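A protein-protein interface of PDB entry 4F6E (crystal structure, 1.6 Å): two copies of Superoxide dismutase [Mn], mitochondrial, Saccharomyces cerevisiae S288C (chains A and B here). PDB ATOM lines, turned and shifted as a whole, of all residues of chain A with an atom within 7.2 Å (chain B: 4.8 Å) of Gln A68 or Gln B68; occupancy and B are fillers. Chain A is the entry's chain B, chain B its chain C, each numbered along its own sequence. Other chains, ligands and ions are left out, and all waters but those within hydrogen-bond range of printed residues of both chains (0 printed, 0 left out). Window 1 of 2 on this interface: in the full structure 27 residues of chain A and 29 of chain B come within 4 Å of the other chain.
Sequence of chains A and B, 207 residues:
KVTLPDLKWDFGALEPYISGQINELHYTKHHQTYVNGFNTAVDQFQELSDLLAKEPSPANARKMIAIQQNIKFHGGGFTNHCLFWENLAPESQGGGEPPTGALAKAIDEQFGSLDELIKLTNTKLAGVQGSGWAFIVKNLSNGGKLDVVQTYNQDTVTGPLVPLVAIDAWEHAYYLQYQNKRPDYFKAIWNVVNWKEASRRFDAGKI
The backbone carbonyl oxygen (O) of Ile A65 sits close to the side-chain amide nitrogen (NE2) of Gln A68, at 3.1 Å.
NE2 of Gln B68 is in hydrogen-bond range of O of Met B64, 3.0 Å away.
Gln B68 touches its own counterpart, Gln A68.
Gln A68 touches MLY B72, but with the chains exchanged MLY A72 does not touch Gln B68 (4.2 Å).
Ile A71 touches Gln B68, but with the chains exchanged Gln A68 does not touch Ile B71 (4.4 Å).
MLY A72 touches Gln B69, but with the chains exchanged Gln A69 does not touch MLY B72 (5.9 Å).
Of the 5 pairs that touch across the chains among the printed residues, 1 has its exchanged pair printed and touching as well.
Ile B71 touches Phe A45 (CG2 to CZ, 3.6 Å).
Gln A68 touches Gln B68 (CB to OE1, 3.2 Å).
NE2 of Gln A68 touches CD of MLY B72, 3.3 Å away.
Ile A71 touches Gln B68 (CG2 to CD, 3.3 Å).
CG of Gln B69 touches CH1 of MLY A72, at 3.9 Å.
Gln A68 touches just these residues of chain B: Gln B68 and MLY B72.
Gln B68 touches just these residues of chain A: Gln A68 (3.2 Å) and Ile A71 (3.3 Å).
Of the printed residues of chain B, Phe A45 touches Ile B71.
Printed residues of chain A within 4 Å of MLY B72: Gln A68.
Of the printed residues of chain B, Ile A71 touches Gln B68.
Of the printed residues of chain B, MLY A72 touches Gln B69 (3.9 Å).
The nearest residue of chain B that does not touch Gln A68 is Ile B71 (4.4 Å).
The nearest printed residue of chain B that does not touch Ile A71 is Ile B65 (4.5 Å).
Of the 9 printed residues of chain B, 4 touch a printed residue of chain A.
Printed residues of chain B that touch a printed residue of chain A: Gln B68, Gln B69, Ile B71 and MLY B72.
Of the 16 printed residues of chain A, 4 touch a printed residue of chain B.
Printed residues of chain A that touch a printed residue of chain B: Phe A45, Gln A68, Ile A71 and MLY A72.
Hydrophobic or aromatic side chains of chain A that line the printed part of chain B: Phe A45 and Ile A71.
Among the printed residues, no Asp or Glu carboxylate lies within 4 Å of a Lys or Arg side-chain nitrogen of the other chain.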
ATOM      1  N   PHE A  38      -6.954  21.549  13.640  1.00  0.00           N
ATOM      2  CA  PHE A  38      -8.380  21.273  13.717  1.00  0.00           C
ATOM      3  C   PHE A  38      -8.610  20.024  14.563  1.00  0.00           C
ATOM      4  O   PHE A  38      -9.473  20.011  15.432  1.00  0.00           O
ATOM      5  CB  PHE A  38      -8.967  21.112  12.307  1.00  0.00           C
ATOM      6  CG  PHE A  38     -10.452  20.900  12.278  1.00  0.00           C
ATOM      7  CD1 PHE A  38     -11.310  21.801  12.880  1.00  0.00           C
ATOM      8  CD2 PHE A  38     -10.994  19.816  11.602  1.00  0.00           C
ATOM      9  CE1 PHE A  38     -12.685  21.612  12.825  1.00  0.00           C
ATOM     10  CE2 PHE A  38     -12.364  19.622  11.548  1.00  0.00           C
ATOM     11  CZ  PHE A  38     -13.210  20.522  12.162  1.00  0.00           C
ATOM     12  N   ALA A  41      -8.088  20.955  18.175  1.00  0.00           N
ATOM     13  CA  ALA A  41      -9.143  21.809  18.710  1.00  0.00           C
ATOM     14  C   ALA A  41     -10.414  21.009  18.994  1.00  0.00           C
ATOM     15  O   ALA A  41     -11.069  21.206  20.016  1.00  0.00           O
ATOM     16  CB  ALA A  41      -9.440  22.952  17.740  1.00  0.00           C
ATOM     17  N   VAL A  42     -10.772  20.117  18.080  1.00  0.00           N
ATOM     18  CA  VAL A  42     -11.972  19.311  18.261  1.00  0.00           C
ATOM     19  C   VAL A  42     -11.808  18.358  19.455  1.00  0.00           C
ATOM     20  O   VAL A  42     -12.729  18.207  20.254  1.00  0.00           O
ATOM     21  CB  VAL A  42     -12.361  18.556  16.971  1.00  0.00           C
ATOM     22  CG1 VAL A  42     -13.478  17.547  17.248  1.00  0.00           C
ATOM     23  CG2 VAL A  42     -12.801  19.554  15.898  1.00  0.00           C
ATOM     24  N   PHE A  45     -12.136  20.452  22.626  1.00  0.00           N
ATOM     25  CA  PHE A  45     -13.510  20.823  22.914  1.00  0.00           C
ATOM     26  C   PHE A  45     -14.293  19.619  23.463  1.00  0.00           C
ATOM     27  O   PHE A  45     -15.081  19.755  24.400  1.00  0.00           O
ATOM     28  CB  PHE A  45     -14.185  21.424  21.685  1.00  0.00           C
ATOM     29  CG  PHE A  45     -15.271  22.410  22.018  1.00  0.00           C
ATOM     30  CD1 PHE A  45     -14.989  23.769  22.109  1.00  0.00           C
ATOM     31  CD2 PHE A  45     -16.569  21.979  22.246  1.00  0.00           C
ATOM     32  CE1 PHE A  45     -15.989  24.676  22.414  1.00  0.00           C
ATOM     33  CE2 PHE A  45     -17.573  22.883  22.551  1.00  0.00           C
ATOM     34  CZ  PHE A  45     -17.280  24.233  22.639  1.00  0.00           C
ATOM     35  N   MLY A  63     -13.425  28.490  29.236  1.00  0.00           N
ATOM     36  CA  MLY A  63     -12.412  27.686  28.546  1.00  0.00           C
ATOM     37  CB  MLY A  63     -12.023  26.471  29.383  1.00  0.00           C
ATOM     38  CG  MLY A  63     -11.245  26.847  30.624  1.00  0.00           C
ATOM     39  CD  MLY A  63     -10.829  25.617  31.399  1.00  0.00           C
ATOM     40  CE  MLY A  63     -10.166  26.008  32.709  1.00  0.00           C
ATOM     41  NZ  MLY A  63      -9.463  24.865  33.351  1.00  0.00           N
ATOM     42  CH1 MLY A  63     -10.400  23.730  33.410  1.00  0.00           C
ATOM     43  CH2 MLY A  63      -9.207  25.280  34.737  1.00  0.00           C
ATOM     44  C   MLY A  63     -12.870  27.247  27.156  1.00  0.00           C
ATOM     45  O   MLY A  63     -12.088  27.273  26.195  1.00  0.00           O
ATOM     46  N   MET A  64     -14.143  26.880  27.050  1.00  0.00           N
ATOM     47  CA  MET A  64     -14.722  26.490  25.765  1.00  0.00           C
ATOM     48  C   MET A  64     -14.781  27.633  24.750  1.00  0.00           C
ATOM     49  O   MET A  64     -14.550  27.415  23.561  1.00  0.00           O
ATOM     50  CB  MET A  64     -16.098  25.861  25.973  1.00  0.00           C
ATOM     51  CG  MET A  64     -16.013  24.530  26.654  1.00  0.00           C
ATOM     52  SD  MET A  64     -17.563  24.027  27.400  1.00  0.00           S
ATOM     53  CE  MET A  64     -18.539  23.753  25.928  1.00  0.00           C
ATOM     54  N   ILE A  65     -15.072  28.844  25.220  1.00  0.00           N
ATOM     55  CA  ILE A  65     -15.049  30.029  24.367  1.00  0.00           C
ATOM     56  C   ILE A  65     -13.663  30.217  23.757  1.00  0.00           C
ATOM     57  O   ILE A  65     -13.523  30.531  22.583  1.00  0.00           O
ATOM     58  CB  ILE A  65     -15.421  31.294  25.168  1.00  0.00           C
ATOM     59  CG1 ILE A  65     -16.863  31.190  25.660  1.00  0.00           C
ATOM     60  CG2 ILE A  65     -15.174  32.561  24.344  1.00  0.00           C
ATOM     61  CD1 ILE A  65     -17.290  32.374  26.523  1.00  0.00           C
ATOM     62  N   ALA A  66     -12.628  30.013  24.563  1.00  0.00           N
ATOM     63  CA  ALA A  66     -11.269  30.185  24.074  1.00  0.00           C
ATOM     64  C   ALA A  66     -10.925  29.198  22.957  1.00  0.00           C
ATOM     65  O   ALA A  66     -10.227  29.547  22.012  1.00  0.00           O
ATOM     66  CB  ALA A  66     -10.274  30.062  25.227  1.00  0.00           C
ATOM     67  N   ILE A  67     -11.432  27.972  23.054  1.00  0.00           N
ATOM     68  CA  ILE A  67     -11.111  26.925  22.076  1.00  0.00           C
ATOM     69  C   ILE A  67     -11.848  27.112  20.747  1.00  0.00           C
ATOM     70  O   ILE A  67     -11.348  26.717  19.690  1.00  0.00           O
ATOM     71  CB  ILE A  67     -11.405  25.508  22.648  1.00  0.00           C
ATOM     72  CG1 ILE A  67     -10.491  25.220  23.837  1.00  0.00           C
ATOM     73  CG2 ILE A  67     -11.183  24.421  21.604  1.00  0.00           C
ATOM     74  CD1 ILE A  67      -9.033  25.461  23.543  1.00  0.00           C
ATOM     75  N   GLN A  68     -13.033  27.705  20.782  1.00  0.00           N
ATOM     76  CA  GLN A  68     -13.800  27.823  19.538  1.00  0.00           C
ATOM     77  C   GLN A  68     -13.076  28.643  18.462  1.00  0.00           C
ATOM     78  O   GLN A  68     -13.254  28.396  17.267  1.00  0.00           O
ATOM     79  CB  GLN A  68     -15.235  28.306  19.781  1.00  0.00           C
ATOM     80  CG  GLN A  68     -15.371  29.665  20.399  1.00  0.00           C
ATOM     81  CD  GLN A  68     -15.067  30.795  19.436  1.00  0.00           C
ATOM     82  OE1 GLN A  68     -15.396  30.730  18.244  1.00  0.00           O
ATOM     83  NE2 GLN A  68     -14.430  31.842  19.948  1.00  0.00           N
ATOM     84  N   GLN A  69     -12.239  29.590  18.875  1.00  0.00           N
ATOM     85  CA  GLN A  69     -11.465  30.376  17.920  1.00  0.00           C
ATOM     86  C   GLN A  69     -10.585  29.457  17.066  1.00  0.00           C
ATOM     87  O   GLN A  69     -10.490  29.631  15.836  1.00  0.00           O
ATOM     88  CB  GLN A  69     -10.601  31.412  18.645  1.00  0.00           C
ATOM     89  CG  GLN A  69      -9.731  32.245  17.717  1.00  0.00           C
ATOM     90  CD  GLN A  69      -8.875  33.254  18.464  1.00  0.00           C
ATOM     91  OE1 GLN A  69      -9.183  33.633  19.596  1.00  0.00           O
ATOM     92  NE2 GLN A  69      -7.792  33.693  17.831  1.00  0.00           N
ATOM     93  N   ASN A  70      -9.958  28.480  17.713  1.00  0.00           N
ATOM     94  CA  ASN A  70      -9.094  27.537  17.003  1.00  0.00           C
ATOM     95  C   ASN A  70      -9.894  26.577  16.137  1.00  0.00           C
ATOM     96  O   ASN A  70      -9.430  26.170  15.067  1.00  0.00           O
ATOM     97  CB  ASN A  70      -8.191  26.777  17.974  1.00  0.00           C
ATOM     98  CG  ASN A  70      -7.205  27.687  18.678  1.00  0.00           C
ATOM     99  OD1 ASN A  70      -6.912  28.788  18.207  1.00  0.00           O
ATOM    100  ND2 ASN A  70      -6.677  27.227  19.811  1.00  0.00           N
ATOM    101  N   ILE A  71     -11.089  26.202  16.588  1.00  0.00           N
ATOM    102  CA  ILE A  71     -11.955  25.361  15.768  1.00  0.00           C
ATOM    103  C   ILE A  71     -12.307  26.092  14.471  1.00  0.00           C
ATOM    104  O   ILE A  71     -12.200  25.520  13.376  1.00  0.00           O
ATOM    105  CB  ILE A  71     -13.251  24.967  16.504  1.00  0.00           C
ATOM    106  CG1 ILE A  71     -12.916  24.124  17.732  1.00  0.00           C
ATOM    107  CG2 ILE A  71     -14.171  24.195  15.559  1.00  0.00           C
ATOM    108  CD1 ILE A  71     -14.117  23.683  18.518  1.00  0.00           C
ATOM    109  N   MLY A  72     -12.700  27.359  14.591  1.00  0.00           N
ATOM    110  CA  MLY A  72     -13.049  28.171  13.421  1.00  0.00           C
ATOM    111  CB  MLY A  72     -13.599  29.527  13.852  1.00  0.00           C
ATOM    112  CG  MLY A  72     -14.105  30.373  12.690  1.00  0.00           C
ATOM    113  CD  MLY A  72     -14.622  31.732  13.147  1.00  0.00           C
ATOM    114  CE  MLY A  72     -15.055  32.569  11.948  1.00  0.00           C
ATOM    115  NZ  MLY A  72     -15.820  33.793  12.320  1.00  0.00           N
ATOM    116  CH1 MLY A  72     -16.879  33.385  13.261  1.00  0.00           C
ATOM    117  CH2 MLY A  72     -14.887  34.688  13.017  1.00  0.00           C
ATOM    118  C   MLY A  72     -11.876  28.377  12.467  1.00  0.00           C
ATOM    119  O   MLY A  72     -12.017  28.182  11.252  1.00  0.00           O
ATOM    120  N   PHE A  73     -10.720  28.756  13.012  1.00  0.00           N
ATOM    121  CA  PHE A  73      -9.562  29.075  12.180  1.00  0.00           C
ATOM    122  C   PHE A  73      -8.993  27.833  11.503  1.00  0.00           C
ATOM    123  O   PHE A  73      -8.815  27.798  10.276  1.00  0.00           O
ATOM    124  CB  PHE A  73      -8.476  29.756  13.017  1.00  0.00           C
ATOM    125  CG  PHE A  73      -7.222  30.050  12.254  1.00  0.00           C
ATOM    126  CD1 PHE A  73      -7.207  31.042  11.288  1.00  0.00           C
ATOM    127  CD2 PHE A  73      -6.061  29.344  12.507  1.00  0.00           C
ATOM    128  CE1 PHE A  73      -6.049  31.327  10.583  1.00  0.00           C
ATOM    129  CE2 PHE A  73      -4.895  29.625  11.808  1.00  0.00           C
ATOM    130  CZ  PHE A  73      -4.889  30.611  10.846  1.00  0.00           C
ATOM    131  N   HIS A  74      -8.709  26.802  12.288  1.00  0.00           N
ATOM    132  CA  HIS A  74      -8.139  25.588  11.704  1.00  0.00           C
ATOM    133  C   HIS A  74      -9.143  24.803  10.892  1.00  0.00           C
ATOM    134  O   HIS A  74      -8.783  24.195   9.877  1.00  0.00           O
ATOM    135  CB  HIS A  74      -7.490  24.707  12.772  1.00  0.00           C
ATOM    136  CG  HIS A  74      -6.255  25.313  13.347  1.00  0.00           C
ATOM    137  ND1 HIS A  74      -5.123  25.546  12.596  1.00  0.00           N
ATOM    138  CD2 HIS A  74      -5.987  25.784  14.588  1.00  0.00           C
ATOM    139  CE1 HIS A  74      -4.201  26.110  13.356  1.00  0.00           C
ATOM    140  NE2 HIS A  74      -4.699  26.262  14.570  1.00  0.00           N
ATOM    141  N   MET B  64     -19.468  22.171  11.329  1.00  0.00           N
ATOM    142  CA  MET B  64     -18.862  22.457  12.623  1.00  0.00           C
ATOM    143  C   MET B  64     -18.448  23.921  12.758  1.00  0.00           C
ATOM    144  O   MET B  64     -18.685  24.552  13.788  1.00  0.00           O
ATOM    145  CB  MET B  64     -17.663  21.543  12.838  1.00  0.00           C
ATOM    146  CG  MET B  64     -17.882  20.522  13.904  1.00  0.00           C
ATOM    147  SD  MET B  64     -17.642  21.113  15.599  1.00  0.00           S
ATOM    148  CE  MET B  64     -17.202  19.498  16.239  1.00  0.00           C
ATOM    149  N   ILE B  65     -17.843  24.471  11.708  1.00  0.00           N
ATOM    150  CA  ILE B  65     -17.481  25.884  11.699  1.00  0.00           C
ATOM    151  C   ILE B  65     -18.703  26.766  11.931  1.00  0.00           C
ATOM    152  O   ILE B  65     -18.652  27.750  12.664  1.00  0.00           O
ATOM    153  CB  ILE B  65     -16.818  26.265  10.351  1.00  0.00           C
ATOM    154  CG1 ILE B  65     -15.471  25.560  10.217  1.00  0.00           C
ATOM    155  CG2 ILE B  65     -16.665  27.768  10.219  1.00  0.00           C
ATOM    156  CD1 ILE B  65     -14.892  25.649   8.813  1.00  0.00           C
ATOM    157  N   ALA B  66     -19.817  26.397  11.311  1.00  0.00           N
ATOM    158  CA  ALA B  66     -21.023  27.202  11.402  1.00  0.00           C
ATOM    159  C   ALA B  66     -21.552  27.326  12.828  1.00  0.00           C
ATOM    160  O   ALA B  66     -22.160  28.336  13.178  1.00  0.00           O
ATOM    161  CB  ALA B  66     -22.103  26.633  10.480  1.00  0.00           C
ATOM    162  N   ILE B  67     -21.326  26.299  13.647  1.00  0.00           N
ATOM    163  CA  ILE B  67     -21.874  26.268  15.016  1.00  0.00           C
ATOM    164  C   ILE B  67     -20.979  27.017  16.016  1.00  0.00           C
ATOM    165  O   ILE B  67     -21.425  27.415  17.104  1.00  0.00           O
ATOM    166  CB  ILE B  67     -22.133  24.811  15.452  1.00  0.00           C
ATOM    167  CG1 ILE B  67     -23.140  24.193  14.479  1.00  0.00           C
ATOM    168  CG2 ILE B  67     -22.644  24.711  16.889  1.00  0.00           C
ATOM    169  CD1 ILE B  67     -23.831  22.996  14.985  1.00  0.00           C
ATOM    170  N   GLN B  68     -19.730  27.245  15.625  1.00  0.00           N
ATOM    171  CA  GLN B  68     -18.759  27.912  16.490  1.00  0.00           C
ATOM    172  C   GLN B  68     -19.230  29.282  16.943  1.00  0.00           C
ATOM    173  O   GLN B  68     -19.000  29.659  18.094  1.00  0.00           O
ATOM    174  CB  GLN B  68     -17.413  28.064  15.779  1.00  0.00           C
ATOM    175  CG  GLN B  68     -16.747  26.759  15.489  1.00  0.00           C
ATOM    176  CD  GLN B  68     -16.828  25.824  16.676  1.00  0.00           C
ATOM    177  OE1 GLN B  68     -16.330  26.133  17.759  1.00  0.00           O
ATOM    178  NE2 GLN B  68     -17.471  24.678  16.483  1.00  0.00           N
ATOM    179  N   GLN B  69     -19.887  30.030  16.056  1.00  0.00           N
ATOM    180  CA  GLN B  69     -20.303  31.381  16.426  1.00  0.00           C
ATOM    181  C   GLN B  69     -21.337  31.353  17.542  1.00  0.00           C
ATOM    182  O   GLN B  69     -21.301  32.200  18.434  1.00  0.00           O
ATOM    183  CB  GLN B  69     -20.833  32.194  15.240  1.00  0.00           C
ATOM    184  CG  GLN B  69     -20.294  33.639  15.185  1.00  0.00           C
ATOM    185  CD  GLN B  69     -20.704  34.530  16.369  1.00  0.00           C
ATOM    186  OE1 GLN B  69     -21.615  35.351  16.253  1.00  0.00           O
ATOM    187  NE2 GLN B  69     -20.002  34.397  17.498  1.00  0.00           N
ATOM    188  N   ASN B  70     -22.252  30.388  17.488  1.00  0.00           N
ATOM    189  CA  ASN B  70     -23.246  30.226  18.551  1.00  0.00           C
ATOM    190  C   ASN B  70     -22.619  29.821  19.883  1.00  0.00           C
ATOM    191  O   ASN B  70     -23.041  30.296  20.944  1.00  0.00           O
ATOM    192  CB  ASN B  70     -24.343  29.238  18.142  1.00  0.00           C
ATOM    193  CG  ASN B  70     -25.189  29.753  16.997  1.00  0.00           C
ATOM    194  OD1 ASN B  70     -25.247  30.958  16.748  1.00  0.00           O
ATOM    195  ND2 ASN B  70     -25.848  28.843  16.290  1.00  0.00           N
ATOM    196  N   ILE B  71     -21.612  28.951  19.837  1.00  0.00           N
ATOM    197  CA  ILE B  71     -20.888  28.575  21.047  1.00  0.00           C
ATOM    198  C   ILE B  71     -20.243  29.813  21.663  1.00  0.00           C
ATOM    199  O   ILE B  71     -20.366  30.051  22.880  1.00  0.00           O
ATOM    200  CB  ILE B  71     -19.804  27.515  20.757  1.00  0.00           C
ATOM    201  CG1 ILE B  71     -20.451  26.192  20.349  1.00  0.00           C
ATOM    202  CG2 ILE B  71     -18.924  27.320  21.976  1.00  0.00           C
ATOM    203  CD1 ILE B  71     -19.456  25.129  19.964  1.00  0.00           C
ATOM    204  N   MLY B  72     -19.595  30.622  20.822  1.00  0.00           N
ATOM    205  CA  MLY B  72     -18.923  31.837  21.291  1.00  0.00           C
ATOM    206  CB  MLY B  72     -18.094  32.468  20.175  1.00  0.00           C
ATOM    207  CG  MLY B  72     -17.365  33.736  20.611  1.00  0.00           C
ATOM    208  CD  MLY B  72     -16.507  34.321  19.487  1.00  0.00           C
ATOM    209  CE  MLY B  72     -15.736  35.545  19.973  1.00  0.00           C
ATOM    210  NZ  MLY B  72     -14.836  36.103  18.926  1.00  0.00           N
ATOM    211  CH1 MLY B  72     -13.978  37.102  19.584  1.00  0.00           C
ATOM    212  CH2 MLY B  72     -15.687  36.832  17.971  1.00  0.00           C
ATOM    213  C   MLY B  72     -19.899  32.866  21.857  1.00  0.00           C
ATOM    214  O   MLY B  72     -19.712  33.385  22.972  1.00  0.00           O
